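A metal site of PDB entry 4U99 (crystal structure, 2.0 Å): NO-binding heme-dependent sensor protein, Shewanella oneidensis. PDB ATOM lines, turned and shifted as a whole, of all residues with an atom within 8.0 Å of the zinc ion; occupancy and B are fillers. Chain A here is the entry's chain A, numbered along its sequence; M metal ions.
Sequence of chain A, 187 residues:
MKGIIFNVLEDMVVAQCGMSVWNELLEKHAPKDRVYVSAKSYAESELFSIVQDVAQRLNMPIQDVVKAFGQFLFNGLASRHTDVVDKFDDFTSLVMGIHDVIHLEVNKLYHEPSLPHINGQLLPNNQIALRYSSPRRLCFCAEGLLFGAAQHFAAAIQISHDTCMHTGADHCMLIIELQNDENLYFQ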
ATOM      1  N   TYR A 132      11.096  13.947  -4.165  1.00  0.00           N
ATOM      2  CA  TYR A 132      12.234  14.796  -3.843  1.00  0.00           C
ATOM      3  C   TYR A 132      12.462  14.827  -2.338  1.00  0.00           C
ATOM      4  O   TYR A 132      11.514  14.946  -1.564  1.00  0.00           O
ATOM      5  CB  TYR A 132      12.002  16.223  -4.359  1.00  0.00           C
ATOM      6  CG  TYR A 132      12.980  17.254  -3.844  1.00  0.00           C
ATOM      7  CD1 TYR A 132      12.752  17.913  -2.642  1.00  0.00           C
ATOM      8  CD2 TYR A 132      14.113  17.592  -4.566  1.00  0.00           C
ATOM      9  CE1 TYR A 132      13.627  18.858  -2.155  1.00  0.00           C
ATOM     10  CE2 TYR A 132      15.001  18.539  -4.099  1.00  0.00           C
ATOM     11  CZ  TYR A 132      14.754  19.174  -2.894  1.00  0.00           C
ATOM     12  OH  TYR A 132      15.630  20.117  -2.416  1.00  0.00           O
ATOM     13  N   ARG A 137      15.709  21.516   1.395  1.00  0.00           N
ATOM     14  CA  ARG A 137      14.298  21.763   1.104  1.00  0.00           C
ATOM     15  C   ARG A 137      14.104  22.759  -0.044  1.00  0.00           C
ATOM     16  O   ARG A 137      13.386  23.748   0.081  1.00  0.00           O
ATOM     17  CB  ARG A 137      13.590  22.267   2.356  1.00  0.00           C
ATOM     18  CG  ARG A 137      13.784  21.343   3.553  1.00  0.00           C
ATOM     19  CD  ARG A 137      12.685  21.500   4.584  1.00  0.00           C
ATOM     20  NE  ARG A 137      12.707  22.817   5.199  1.00  0.00           N
ATOM     21  CZ  ARG A 137      11.821  23.234   6.100  1.00  0.00           C
ATOM     22  NH1 ARG A 137      10.841  22.415   6.483  1.00  0.00           N
ATOM     23  NH2 ARG A 137      11.912  24.457   6.609  1.00  0.00           N
ATOM     24  N   LEU A 138      14.759  22.465  -1.167  1.00  0.00           N
ATOM     25  CA  LEU A 138      14.725  23.336  -2.345  1.00  0.00           C
ATOM     26  C   LEU A 138      13.802  22.769  -3.417  1.00  0.00           C
ATOM     27  O   LEU A 138      14.108  22.833  -4.609  1.00  0.00           O
ATOM     28  CB  LEU A 138      16.149  23.502  -2.896  1.00  0.00           C
ATOM     29  CG  LEU A 138      17.069  24.389  -2.056  1.00  0.00           C
ATOM     30  CD1 LEU A 138      18.520  24.249  -2.509  1.00  0.00           C
ATOM     31  CD2 LEU A 138      16.617  25.840  -2.142  1.00  0.00           C
ATOM     32  N   CYS A 139      12.666  22.216  -2.986  1.00  0.00           N
ATOM     33  CA  CYS A 139      11.710  21.610  -3.901  1.00  0.00           C
ATOM     34  C   CYS A 139      11.176  22.592  -4.937  1.00  0.00           C
ATOM     35  O   CYS A 139      10.825  22.203  -6.053  1.00  0.00           O
ATOM     36  CB  CYS A 139      10.535  21.006  -3.117  1.00  0.00           C
ATOM     37  SG  CYS A 139       9.706  22.183  -2.010  1.00  0.00           S
ATOM     38  N   PHE A 140      11.118  23.875  -4.590  1.00  0.00           N
ATOM     39  CA  PHE A 140      10.622  24.858  -5.535  1.00  0.00           C
ATOM     40  C   PHE A 140      11.691  25.204  -6.562  1.00  0.00           C
ATOM     41  O   PHE A 140      11.370  25.585  -7.686  1.00  0.00           O
ATOM     42  CB  PHE A 140      10.145  26.103  -4.790  1.00  0.00           C
ATOM     43  CG  PHE A 140       8.833  25.890  -4.079  1.00  0.00           C
ATOM     44  CD1 PHE A 140       7.632  25.970  -4.778  1.00  0.00           C
ATOM     45  CD2 PHE A 140       8.789  25.597  -2.728  1.00  0.00           C
ATOM     46  CE1 PHE A 140       6.422  25.762  -4.147  1.00  0.00           C
ATOM     47  CE2 PHE A 140       7.579  25.392  -2.088  1.00  0.00           C
ATOM     48  CZ  PHE A 140       6.401  25.473  -2.797  1.00  0.00           C
ATOM     49  N   ALA A 142      13.606  22.789  -7.601  1.00  0.00           N
ATOM     50  CA  ALA A 142      13.379  21.609  -8.422  1.00  0.00           C
ATOM     51  C   ALA A 142      12.239  21.817  -9.403  1.00  0.00           C
ATOM     52  O   ALA A 142      12.356  21.457 -10.581  1.00  0.00           O
ATOM     53  CB  ALA A 142      13.111  20.391  -7.547  1.00  0.00           C
ATOM     54  N   GLU A 143      11.137  22.394  -8.924  1.00  0.00           N
ATOM     55  CA  GLU A 143       9.994  22.705  -9.800  1.00  0.00           C
ATOM     56  C   GLU A 143      10.448  23.580 -10.955  1.00  0.00           C
ATOM     57  O   GLU A 143      10.161  23.279 -12.114  1.00  0.00           O
ATOM     58  CB  GLU A 143       8.866  23.411  -9.027  1.00  0.00           C
ATOM     59  CG  GLU A 143       7.686  22.524  -8.716  1.00  0.00           C
ATOM     60  CD  GLU A 143       6.442  23.322  -8.313  1.00  0.00           C
ATOM     61  OE1 GLU A 143       5.936  23.091  -7.198  1.00  0.00           O
ATOM     62  OE2 GLU A 143       5.969  24.147  -9.122  1.00  0.00           O
ATOM     63  N   HIS A 161       2.075  19.622  -6.537  1.00  0.00           N
ATOM     64  CA  HIS A 161       3.096  19.606  -5.484  1.00  0.00           C
ATOM     65  C   HIS A 161       2.379  19.636  -4.128  1.00  0.00           C
ATOM     66  O   HIS A 161       2.481  20.593  -3.375  1.00  0.00           O
ATOM     67  CB  HIS A 161       4.035  20.802  -5.663  1.00  0.00           C
ATOM     68  CG  HIS A 161       5.231  20.808  -4.765  1.00  0.00           C
ATOM     69  ND1 HIS A 161       6.280  21.675  -4.952  1.00  0.00           N
ATOM     70  CD2 HIS A 161       5.530  20.078  -3.668  1.00  0.00           C
ATOM     71  CE1 HIS A 161       7.193  21.476  -4.014  1.00  0.00           C
ATOM     72  NE2 HIS A 161       6.764  20.516  -3.221  1.00  0.00           N
ATOM     73  N   ASP A 162       1.643  18.556  -3.845  1.00  0.00           N
ATOM     74  CA  ASP A 162       0.672  18.540  -2.746  1.00  0.00           C
ATOM     75  C   ASP A 162       1.184  17.811  -1.506  1.00  0.00           C
ATOM     76  O   ASP A 162       0.558  17.870  -0.447  1.00  0.00           O
ATOM     77  CB  ASP A 162      -0.627  17.908  -3.214  1.00  0.00           C
ATOM     78  CG  ASP A 162      -1.320  18.726  -4.287  1.00  0.00           C
ATOM     79  OD1 ASP A 162      -1.381  19.970  -4.136  1.00  0.00           O
ATOM     80  OD2 ASP A 162      -1.776  18.144  -5.293  1.00  0.00           O
ATOM     81  N   THR A 163       2.294  17.099  -1.651  1.00  0.00           N
ATOM     82  CA  THR A 163       3.047  16.590  -0.514  1.00  0.00           C
ATOM     83  C   THR A 163       4.339  17.370  -0.504  1.00  0.00           C
ATOM     84  O   THR A 163       5.029  17.443  -1.523  1.00  0.00           O
ATOM     85  CB  THR A 163       3.318  15.077  -0.612  1.00  0.00           C
ATOM     86  OG1 THR A 163       2.075  14.370  -0.673  1.00  0.00           O
ATOM     87  CG2 THR A 163       4.128  14.590   0.583  1.00  0.00           C
ATOM     88  N   CYS A 164       4.677  17.970   0.630  1.00  0.00           N
ATOM     89  CA  CYS A 164       5.807  18.894   0.657  1.00  0.00           C
ATOM     90  C   CYS A 164       6.462  18.948   2.029  1.00  0.00           C
ATOM     91  O   CYS A 164       5.798  18.890   3.066  1.00  0.00           O
ATOM     92  CB  CYS A 164       5.345  20.288   0.235  1.00  0.00           C
ATOM     93  SG  CYS A 164       6.653  21.532   0.173  1.00  0.00           S
ATOM     94  N   MET A 165       7.792  19.059   2.022  1.00  0.00           N
ATOM     95  CA  MET A 165       8.560  19.137   3.250  1.00  0.00           C
ATOM     96  C   MET A 165       8.177  20.386   4.035  1.00  0.00           C
ATOM     97  O   MET A 165       8.258  20.405   5.257  1.00  0.00           O
ATOM     98  CB  MET A 165      10.058  19.134   2.958  1.00  0.00           C
ATOM     99  CG  MET A 165      10.553  17.859   2.268  1.00  0.00           C
ATOM    100  SD  MET A 165      12.351  17.812   2.026  1.00  0.00           S
ATOM    101  CE  MET A 165      12.902  17.488   3.699  1.00  0.00           C
ATOM    102  N   HIS A 166       7.749  21.423   3.315  1.00  0.00           N
ATOM    103  CA  HIS A 166       7.369  22.680   3.947  1.00  0.00           C
ATOM    104  C   HIS A 166       5.999  22.600   4.617  1.00  0.00           C
ATOM    105  O   HIS A 166       5.656  23.474   5.421  1.00  0.00           O
ATOM    106  CB  HIS A 166       7.371  23.807   2.912  1.00  0.00           C
ATOM    107  CG  HIS A 166       8.740  24.160   2.412  1.00  0.00           C
ATOM    108  ND1 HIS A 166       9.618  24.938   3.148  1.00  0.00           N
ATOM    109  CD2 HIS A 166       9.391  23.822   1.275  1.00  0.00           C
ATOM    110  CE1 HIS A 166      10.742  25.072   2.468  1.00  0.00           C
ATOM    111  NE2 HIS A 166      10.637  24.411   1.335  1.00  0.00           N
ATOM    112  N   THR A 167       5.212  21.574   4.295  1.00  0.00           N
ATOM    113  CA  THR A 167       3.929  21.344   4.959  1.00  0.00           C
ATOM    114  C   THR A 167       4.018  20.125   5.877  1.00  0.00           C
ATOM    115  O   THR A 167       2.990  19.532   6.224  1.00  0.00           O
ATOM    116  CB  THR A 167       2.772  21.157   3.947  1.00  0.00           C
ATOM    117  OG1 THR A 167       3.049  20.049   3.079  1.00  0.00           O
ATOM    118  CG2 THR A 167       2.588  22.422   3.112  1.00  0.00           C
ATOM    119  N   ALA A 169       5.988  17.089   5.673  1.00  0.00           N
ATOM    120  CA  ALA A 169       6.430  15.768   5.254  1.00  0.00           C
ATOM    121  C   ALA A 169       7.956  15.679   5.238  1.00  0.00           C
ATOM    122  O   ALA A 169       8.628  16.704   5.358  1.00  0.00           O
ATOM    123  CB  ALA A 169       5.860  15.438   3.884  1.00  0.00           C
ATOM    124  N   HIS A 171       9.491  14.511   2.658  1.00  0.00           N
ATOM    125  CA  HIS A 171       9.788  14.511   1.233  1.00  0.00           C
ATOM    126  C   HIS A 171       8.703  15.296   0.507  1.00  0.00           C
ATOM    127  O   HIS A 171       7.667  15.619   1.086  1.00  0.00           O
ATOM    128  CB  HIS A 171       9.841  13.082   0.686  1.00  0.00           C
ATOM    129  CG  HIS A 171       8.524  12.389   0.693  1.00  0.00           C
ATOM    130  ND1 HIS A 171       8.004  11.780   1.825  1.00  0.00           N
ATOM    131  CD2 HIS A 171       7.591  12.215  -0.279  1.00  0.00           C
ATOM    132  CE1 HIS A 171       6.827  11.261   1.543  1.00  0.00           C
ATOM    133  NE2 HIS A 171       6.544  11.511   0.278  1.00  0.00           N
ATOM    134  N   CYS A 172       8.958  15.601  -0.763  1.00  0.00           N
ATOM    135  CA  CYS A 172       7.957  16.207  -1.623  1.00  0.00           C
ATOM    136  C   CYS A 172       7.606  15.257  -2.764  1.00  0.00           C
ATOM    137  O   CYS A 172       8.465  14.500  -3.227  1.00  0.00           O
ATOM    138  CB  CYS A 172       8.458  17.539  -2.201  1.00  0.00           C
ATOM    139  SG  CYS A 172       9.049  18.737  -0.985  1.00  0.00           S
ATOM    140  N   MET A 173       6.355  15.299  -3.195  1.00  0.00           N
ATOM    141  CA  MET A 173       5.912  14.567  -4.380  1.00  0.00           C
ATOM    142  C   MET A 173       5.534  15.562  -5.468  1.00  0.00           C
ATOM    143  O   MET A 173       4.564  16.308  -5.337  1.00  0.00           O
ATOM    144  CB  MET A 173       4.725  13.660  -4.076  1.00  0.00           C
ATOM    145  CG  MET A 173       5.046  12.420  -3.254  1.00  0.00           C
ATOM    146  SD  MET A 173       6.311  11.321  -3.965  1.00  0.00           S
ATOM    147  CE  MET A 173       5.807  11.246  -5.687  1.00  0.00           C
ATOM    148  N   LEU A 174       6.325  15.580  -6.547  1.00  0.00           N
ATOM    149  CA  LEU A 174       6.038  16.427  -7.693  1.00  0.00           C
ATOM    150  C   LEU A 174       5.418  15.568  -8.789  1.00  0.00           C
ATOM    151  O   LEU A 174       6.101  14.734  -9.383  1.00  0.00           O
ATOM    152  CB  LEU A 174       7.309  17.115  -8.195  1.00  0.00           C
ATOM    153  CG  LEU A 174       7.771  18.355  -7.422  1.00  0.00           C
ATOM    154  CD1 LEU A 174       7.992  18.050  -5.967  1.00  0.00           C
ATOM    155  CD2 LEU A 174       9.038  18.919  -8.037  1.00  0.00           C
HETATM  156 ZN    ZN M   1       7.985  20.691  -1.579  1.00  0.00          ZN
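The backbone carbonyl oxygen (O) of Met 165 lies within hydrogen-bond range of the guanidinium group (NH1) of Arg 137 (3.5 Å).
N of Cys 172 is in hydrogen-bond range of O of Tyr 132, 2.8 Å away.
O of Cys 164 sits at hydrogen-bond distance from N of Ala 169.
A ring nitrogen (ND1) of His 161 sits at hydrogen-bond distance from the side-chain carboxylate (OE1) of Glu 143.
OG1 of Thr 167 sits at hydrogen-bond distance from O of Cys 164 (3.0 Å).
The backbone NH of Met 165 sits close to the side-chain sulfur of Cys 172, 3.3 Å away.
N of His 166 sits close to SG of Cys 164, 3.3 Å away.
The zinc ion is bound by a ring nitrogen (NE2) of His 161 (2.1 Å), the side-chain sulfur (SG) of Cys 172 (2.3 Å), the side-chain sulfur (SG) of Cys 139 (2.3 Å) and the side-chain sulfur (SG) of Cys 164 (2.4 Å).
Met 165 touches the zinc ion.
Within 4 Å of the zinc ion: Cys 139, His 161, Cys 164, Met 165 and Cys 172.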
